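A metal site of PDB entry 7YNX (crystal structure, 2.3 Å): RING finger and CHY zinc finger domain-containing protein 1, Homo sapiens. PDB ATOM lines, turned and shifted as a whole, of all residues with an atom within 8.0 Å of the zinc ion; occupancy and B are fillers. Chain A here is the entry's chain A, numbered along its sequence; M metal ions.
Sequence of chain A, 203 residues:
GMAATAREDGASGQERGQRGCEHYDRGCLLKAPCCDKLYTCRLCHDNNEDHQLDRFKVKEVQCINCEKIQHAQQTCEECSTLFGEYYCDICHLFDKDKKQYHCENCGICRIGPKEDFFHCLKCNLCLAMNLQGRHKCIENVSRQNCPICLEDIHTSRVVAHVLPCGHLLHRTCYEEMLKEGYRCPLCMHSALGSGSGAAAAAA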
ATOM      1  N   TYR A 101     -11.027  16.581  -1.560  1.00  0.00           N
ATOM      2  CA  TYR A 101     -10.969  17.622  -2.557  1.00  0.00           C
ATOM      3  C   TYR A 101      -9.526  18.055  -2.675  1.00  0.00           C
ATOM      4  O   TYR A 101      -8.737  17.951  -1.727  1.00  0.00           O
ATOM      5  CB  TYR A 101     -11.850  18.820  -2.188  1.00  0.00           C
ATOM      6  CG  TYR A 101     -11.378  19.563  -0.961  1.00  0.00           C
ATOM      7  CD1 TYR A 101     -11.602  19.049   0.294  1.00  0.00           C
ATOM      8  CD2 TYR A 101     -10.676  20.756  -1.061  1.00  0.00           C
ATOM      9  CE1 TYR A 101     -11.164  19.704   1.431  1.00  0.00           C
ATOM     10  CE2 TYR A 101     -10.222  21.426   0.068  1.00  0.00           C
ATOM     11  CZ  TYR A 101     -10.476  20.895   1.311  1.00  0.00           C
ATOM     12  OH  TYR A 101     -10.052  21.540   2.464  1.00  0.00           O
ATOM     13  N   HIS A 102      -9.166  18.524  -3.865  1.00  0.00           N
ATOM     14  CA  HIS A 102      -7.837  19.073  -4.092  1.00  0.00           C
ATOM     15  C   HIS A 102      -7.917  20.588  -3.964  1.00  0.00           C
ATOM     16  O   HIS A 102      -8.742  21.224  -4.631  1.00  0.00           O
ATOM     17  CB  HIS A 102      -7.296  18.680  -5.468  1.00  0.00           C
ATOM     18  CG  HIS A 102      -5.985  19.317  -5.800  1.00  0.00           C
ATOM     19  ND1 HIS A 102      -4.779  18.774  -5.420  1.00  0.00           N
ATOM     20  CD2 HIS A 102      -5.695  20.480  -6.429  1.00  0.00           C
ATOM     21  CE1 HIS A 102      -3.785  19.552  -5.826  1.00  0.00           C
ATOM     22  NE2 HIS A 102      -4.321  20.593  -6.442  1.00  0.00           N
ATOM     23  N   CYS A 103      -7.071  21.148  -3.120  1.00  0.00           N
ATOM     24  CA  CYS A 103      -7.033  22.584  -2.855  1.00  0.00           C
ATOM     25  C   CYS A 103      -5.786  23.170  -3.521  1.00  0.00           C
ATOM     26  O   CYS A 103      -4.670  22.756  -3.215  1.00  0.00           O
ATOM     27  CB  CYS A 103      -7.028  22.858  -1.353  1.00  0.00           C
ATOM     28  SG  CYS A 103      -6.535  24.531  -0.962  1.00  0.00           S
ATOM     29  N   GLU A 104      -5.996  24.145  -4.416  1.00  0.00           N
ATOM     30  CA  GLU A 104      -4.860  24.682  -5.173  1.00  0.00           C
ATOM     31  C   GLU A 104      -3.874  25.430  -4.292  1.00  0.00           C
ATOM     32  O   GLU A 104      -2.675  25.436  -4.585  1.00  0.00           O
ATOM     33  CB  GLU A 104      -5.349  25.616  -6.283  1.00  0.00           C
ATOM     34  CG  GLU A 104      -6.263  24.965  -7.334  1.00  0.00           C
ATOM     35  CD  GLU A 104      -5.502  24.275  -8.471  1.00  0.00           C
ATOM     36  OE1 GLU A 104      -5.859  23.120  -8.808  1.00  0.00           O
ATOM     37  OE2 GLU A 104      -4.562  24.882  -9.038  1.00  0.00           O
ATOM     38  N   ASN A 105      -4.353  26.073  -3.208  1.00  0.00           N
ATOM     39  CA  ASN A 105      -3.470  26.863  -2.348  1.00  0.00           C
ATOM     40  C   ASN A 105      -2.642  25.969  -1.445  1.00  0.00           C
ATOM     41  O   ASN A 105      -1.428  26.218  -1.255  1.00  0.00           O
ATOM     42  CB  ASN A 105      -4.276  27.841  -1.501  1.00  0.00           C
ATOM     43  CG  ASN A 105      -4.982  28.876  -2.323  1.00  0.00           C
ATOM     44  OD1 ASN A 105      -4.348  29.755  -2.914  1.00  0.00           O
ATOM     45  ND2 ASN A 105      -6.304  28.794  -2.371  1.00  0.00           N
ATOM     46  N   CYS A 106      -3.272  24.938  -0.863  1.00  0.00           N
ATOM     47  CA  CYS A 106      -2.501  23.902  -0.188  1.00  0.00           C
ATOM     48  C   CYS A 106      -1.536  23.241  -1.177  1.00  0.00           C
ATOM     49  O   CYS A 106      -0.396  22.944  -0.837  1.00  0.00           O
ATOM     50  CB  CYS A 106      -3.445  22.876   0.435  1.00  0.00           C
ATOM     51  SG  CYS A 106      -4.176  23.384   2.048  1.00  0.00           S
ATOM     52  N   GLY A 107      -1.976  23.062  -2.417  1.00  0.00           N
ATOM     53  CA  GLY A 107      -1.195  22.342  -3.400  1.00  0.00           C
ATOM     54  C   GLY A 107      -1.361  20.853  -3.336  1.00  0.00           C
ATOM     55  O   GLY A 107      -0.688  20.143  -4.107  1.00  0.00           O
ATOM     56  N   ILE A 108      -2.232  20.330  -2.471  1.00  0.00           N
ATOM     57  CA  ILE A 108      -2.403  18.900  -2.291  1.00  0.00           C
ATOM     58  C   ILE A 108      -3.892  18.604  -2.133  1.00  0.00           C
ATOM     59  O   ILE A 108      -4.732  19.516  -2.099  1.00  0.00           O
ATOM     60  CB  ILE A 108      -1.623  18.358  -1.081  1.00  0.00           C
ATOM     61  CG1 ILE A 108      -1.892  19.224   0.164  1.00  0.00           C
ATOM     62  CG2 ILE A 108      -0.122  18.249  -1.387  1.00  0.00           C
ATOM     63  CD1 ILE A 108      -1.426  18.598   1.478  1.00  0.00           C
ATOM     64  N   CYS A 109      -4.208  17.323  -2.009  1.00  0.00           N
ATOM     65  CA  CYS A 109      -5.564  16.917  -1.691  1.00  0.00           C
ATOM     66  C   CYS A 109      -5.797  16.936  -0.179  1.00  0.00           C
ATOM     67  O   CYS A 109      -4.941  16.511   0.600  1.00  0.00           O
ATOM     68  CB  CYS A 109      -5.845  15.517  -2.241  1.00  0.00           C
ATOM     69  SG  CYS A 109      -6.466  15.535  -3.941  1.00  0.00           S
ATOM     70  N   ARG A 110      -6.955  17.444   0.222  1.00  0.00           N
ATOM     71  CA  ARG A 110      -7.375  17.461   1.605  1.00  0.00           C
ATOM     72  C   ARG A 110      -8.487  16.437   1.843  1.00  0.00           C
ATOM     73  O   ARG A 110      -9.181  16.019   0.914  1.00  0.00           O
ATOM     74  CB  ARG A 110      -7.853  18.857   2.000  1.00  0.00           C
ATOM     75  CG  ARG A 110      -6.730  19.894   2.085  1.00  0.00           C
ATOM     76  CD  ARG A 110      -5.793  19.572   3.251  1.00  0.00           C
ATOM     77  NE  ARG A 110      -4.624  20.442   3.254  1.00  0.00           N
ATOM     78  CZ  ARG A 110      -3.579  20.273   4.048  1.00  0.00           C
ATOM     79  NH1 ARG A 110      -3.567  19.264   4.916  1.00  0.00           N
ATOM     80  NH2 ARG A 110      -2.556  21.103   3.957  1.00  0.00           N
ATOM     81  N   LYS A 114     -15.392  19.637   1.279  1.00  0.00           N
ATOM     82  CA  LYS A 114     -14.784  20.927   0.978  1.00  0.00           C
ATOM     83  C   LYS A 114     -15.526  22.089   1.650  1.00  0.00           C
ATOM     84  O   LYS A 114     -14.926  23.136   1.908  1.00  0.00           O
ATOM     85  CB  LYS A 114     -14.735  21.144  -0.539  1.00  0.00           C
ATOM     86  CG  LYS A 114     -13.719  22.211  -0.966  1.00  0.00           C
ATOM     87  CD  LYS A 114     -14.350  23.523  -1.423  1.00  0.00           C
ATOM     88  CE  LYS A 114     -13.282  24.601  -1.737  1.00  0.00           C
ATOM     89  NZ  LYS A 114     -12.393  25.001  -0.572  1.00  0.00           N
ATOM     90  N   PHE A 117     -14.487  23.592   5.132  1.00  0.00           N
ATOM     91  CA  PHE A 117     -13.178  24.195   5.245  1.00  0.00           C
ATOM     92  C   PHE A 117     -13.084  25.442   4.372  1.00  0.00           C
ATOM     93  O   PHE A 117     -13.824  25.617   3.411  1.00  0.00           O
ATOM     94  CB  PHE A 117     -12.094  23.185   4.854  1.00  0.00           C
ATOM     95  CG  PHE A 117     -12.040  22.003   5.764  1.00  0.00           C
ATOM     96  CD1 PHE A 117     -11.519  22.131   7.054  1.00  0.00           C
ATOM     97  CD2 PHE A 117     -12.550  20.780   5.359  1.00  0.00           C
ATOM     98  CE1 PHE A 117     -11.498  21.051   7.910  1.00  0.00           C
ATOM     99  CE2 PHE A 117     -12.523  19.678   6.213  1.00  0.00           C
ATOM    100  CZ  PHE A 117     -11.987  19.821   7.495  1.00  0.00           C
ATOM    101  N   PHE A 118     -12.165  26.323   4.781  1.00  0.00           N
ATOM    102  CA  PHE A 118     -11.716  27.441   3.975  1.00  0.00           C
ATOM    103  C   PHE A 118     -10.193  27.470   4.033  1.00  0.00           C
ATOM    104  O   PHE A 118      -9.597  27.070   5.039  1.00  0.00           O
ATOM    105  CB  PHE A 118     -12.285  28.787   4.476  1.00  0.00           C
ATOM    106  CG  PHE A 118     -11.547  29.345   5.669  1.00  0.00           C
ATOM    107  CD1 PHE A 118     -11.811  28.869   6.943  1.00  0.00           C
ATOM    108  CD2 PHE A 118     -10.571  30.312   5.509  1.00  0.00           C
ATOM    109  CE1 PHE A 118     -11.126  29.371   8.055  1.00  0.00           C
ATOM    110  CE2 PHE A 118      -9.881  30.821   6.606  1.00  0.00           C
ATOM    111  CZ  PHE A 118     -10.149  30.354   7.877  1.00  0.00           C
ATOM    112  N   HIS A 119      -9.568  27.924   2.964  1.00  0.00           N
ATOM    113  CA  HIS A 119      -8.122  28.065   2.977  1.00  0.00           C
ATOM    114  C   HIS A 119      -7.768  29.440   3.534  1.00  0.00           C
ATOM    115  O   HIS A 119      -8.232  30.464   3.030  1.00  0.00           O
ATOM    116  CB  HIS A 119      -7.525  27.883   1.579  1.00  0.00           C
ATOM    117  CG  HIS A 119      -6.035  27.756   1.600  1.00  0.00           C
ATOM    118  ND1 HIS A 119      -5.384  26.547   1.647  1.00  0.00           N
ATOM    119  CD2 HIS A 119      -5.063  28.708   1.656  1.00  0.00           C
ATOM    120  CE1 HIS A 119      -4.085  26.739   1.702  1.00  0.00           C
ATOM    121  NE2 HIS A 119      -3.858  28.048   1.704  1.00  0.00           N
ATOM    122  N   CYS A 120      -6.962  29.458   4.590  1.00  0.00           N
ATOM    123  CA  CYS A 120      -6.441  30.718   5.099  1.00  0.00           C
ATOM    124  C   CYS A 120      -5.167  31.057   4.343  1.00  0.00           C
ATOM    125  O   CYS A 120      -4.196  30.294   4.399  1.00  0.00           O
ATOM    126  CB  CYS A 120      -6.154  30.641   6.596  1.00  0.00           C
ATOM    127  SG  CYS A 120      -5.363  32.151   7.193  1.00  0.00           S
ATOM    128  N   LEU A 121      -5.185  32.183   3.621  1.00  0.00           N
ATOM    129  CA  LEU A 121      -4.008  32.583   2.855  1.00  0.00           C
ATOM    130  C   LEU A 121      -2.780  32.718   3.754  1.00  0.00           C
ATOM    131  O   LEU A 121      -1.704  32.191   3.444  1.00  0.00           O
ATOM    132  CB  LEU A 121      -4.268  33.898   2.130  1.00  0.00           C
ATOM    133  CG  LEU A 121      -5.488  34.021   1.204  1.00  0.00           C
ATOM    134  CD1 LEU A 121      -5.748  35.482   0.853  1.00  0.00           C
ATOM    135  CD2 LEU A 121      -5.328  33.182  -0.067  1.00  0.00           C
ATOM    136  N   ASN A 124      -1.762  29.543   5.468  1.00  0.00           N
ATOM    137  CA  ASN A 124      -1.511  28.787   4.253  1.00  0.00           C
ATOM    138  C   ASN A 124      -1.891  27.312   4.391  1.00  0.00           C
ATOM    139  O   ASN A 124      -1.215  26.446   3.854  1.00  0.00           O
ATOM    140  CB  ASN A 124      -0.072  28.931   3.782  1.00  0.00           C
ATOM    141  CG  ASN A 124       0.012  29.054   2.283  1.00  0.00           C
ATOM    142  OD1 ASN A 124      -0.991  28.892   1.601  1.00  0.00           O
ATOM    143  ND2 ASN A 124       1.208  29.354   1.759  1.00  0.00           N
ATOM    144  N   LEU A 125      -2.999  27.043   5.070  1.00  0.00           N
ATOM    145  CA  LEU A 125      -3.616  25.719   5.025  1.00  0.00           C
ATOM    146  C   LEU A 125      -5.131  25.883   5.089  1.00  0.00           C
ATOM    147  O   LEU A 125      -5.658  26.976   5.305  1.00  0.00           O
ATOM    148  CB  LEU A 125      -3.130  24.802   6.149  1.00  0.00           C
ATOM    149  CG  LEU A 125      -3.724  24.938   7.545  1.00  0.00           C
ATOM    150  CD1 LEU A 125      -3.112  23.865   8.423  1.00  0.00           C
ATOM    151  CD2 LEU A 125      -3.481  26.314   8.131  1.00  0.00           C
ATOM    152  N   CYS A 126      -5.834  24.758   4.883  1.00  0.00           N
ATOM    153  CA  CYS A 126      -7.289  24.746   4.967  1.00  0.00           C
ATOM    154  C   CYS A 126      -7.744  24.577   6.413  1.00  0.00           C
ATOM    155  O   CYS A 126      -7.256  23.687   7.130  1.00  0.00           O
ATOM    156  CB  CYS A 126      -7.866  23.627   4.102  1.00  0.00           C
ATOM    157  SG  CYS A 126      -8.157  24.102   2.372  1.00  0.00           S
ATOM    158  N   LEU A 127      -8.691  25.414   6.839  1.00  0.00           N
ATOM    159  CA  LEU A 127      -9.159  25.440   8.209  1.00  0.00           C
ATOM    160  C   LEU A 127     -10.670  25.274   8.256  1.00  0.00           C
ATOM    161  O   LEU A 127     -11.385  25.657   7.321  1.00  0.00           O
ATOM    162  CB  LEU A 127      -8.765  26.753   8.912  1.00  0.00           C
ATOM    163  CG  LEU A 127      -7.262  26.922   9.183  1.00  0.00           C
ATOM    164  CD1 LEU A 127      -6.978  28.162  10.013  1.00  0.00           C
ATOM    165  CD2 LEU A 127      -6.744  25.690   9.886  1.00  0.00           C
ATOM    166  N   ARG A 143       3.422  25.562   6.995  1.00  0.00           N
ATOM    167  CA  ARG A 143       4.562  25.021   6.258  1.00  0.00           C
ATOM    168  C   ARG A 143       5.746  24.796   7.168  1.00  0.00           C
ATOM    169  O   ARG A 143       6.890  25.021   6.790  1.00  0.00           O
ATOM    170  CB  ARG A 143       4.932  25.945   5.094  1.00  0.00           C
ATOM    171  CG  ARG A 143       3.781  26.405   4.188  1.00  0.00           C
ATOM    172  CD  ARG A 143       2.917  25.245   3.669  1.00  0.00           C
ATOM    173  NE  ARG A 143       1.726  25.724   2.955  1.00  0.00           N
ATOM    174  CZ  ARG A 143       1.579  25.673   1.626  1.00  0.00           C
ATOM    175  NH1 ARG A 143       2.545  25.186   0.855  1.00  0.00           N
ATOM    176  NH2 ARG A 143       0.468  26.130   1.058  1.00  0.00           N
ATOM    177  N   HIS A 154       1.932  20.455   7.255  1.00  0.00           N
ATOM    178  CA  HIS A 154       1.115  20.804   6.090  1.00  0.00           C
ATOM    179  C   HIS A 154       0.684  19.577   5.296  1.00  0.00           C
ATOM    180  O   HIS A 154      -0.474  19.473   4.874  1.00  0.00           O
ATOM    181  CB  HIS A 154       1.884  21.755   5.183  1.00  0.00           C
ATOM    182  CG  HIS A 154       1.085  22.249   4.017  1.00  0.00           C
ATOM    183  ND1 HIS A 154       0.088  23.185   4.149  1.00  0.00           N
ATOM    184  CD2 HIS A 154       1.138  21.948   2.699  1.00  0.00           C
ATOM    185  CE1 HIS A 154      -0.439  23.445   2.960  1.00  0.00           C
ATOM    186  NE2 HIS A 154       0.189  22.702   2.075  1.00  0.00           N
ATOM    187  N   ALA A 200      -7.977  20.834   8.040  1.00  0.00           N
ATOM    188  CA  ALA A 200      -8.249  19.695   7.163  1.00  0.00           C
ATOM    189  C   ALA A 200      -7.025  18.810   7.015  1.00  0.00           C
ATOM    190  O   ALA A 200      -5.901  19.298   6.840  1.00  0.00           O
ATOM    191  CB  ALA A 200      -8.702  20.171   5.785  1.00  0.00           C
HETATM  192 ZN    ZN M   1      -5.958  24.625   1.405  1.00  0.00          ZN
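The guanidinium group of Arg 110 lies close to the side-chain sulfur of Cys 106 (3.2 Å). SG of Cys 103 lies close to N of Asn 105, 3.5 Å away. OH of Tyr 101 sits close to SG of Cys 126 (3.2 Å). O of Cys 106 sits at hydrogen-bond distance from NE2 of His 154 (3.0 Å). N of Cys 120 lies within hydrogen-bond range of O of Leu 125 (2.9 Å). NE2 of His 119 is in hydrogen-bond range of OD1 of Asn 124. N of Cys 103 lies within hydrogen-bond range of O of Ile 108, at 3.0 Å. O of Cys 126 is in hydrogen-bond range of N of Ala 200.
Leu 125 touches the zinc ion (C to ZN, 3.98 Å). Of the 23 residues printed, 5 come within 4 Å of the zinc ion.
The zinc ion is bound by ND1 of His 119 (2.0 Å). The zinc ion is bound by the side-chain sulfur (SG) of Cys 106 (2.3 Å). The zinc ion is bound by the side-chain sulfur (SG) of Cys 103 (2.4 Å). The zinc ion is bound by the side-chain sulfur (SG) of Cys 126.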
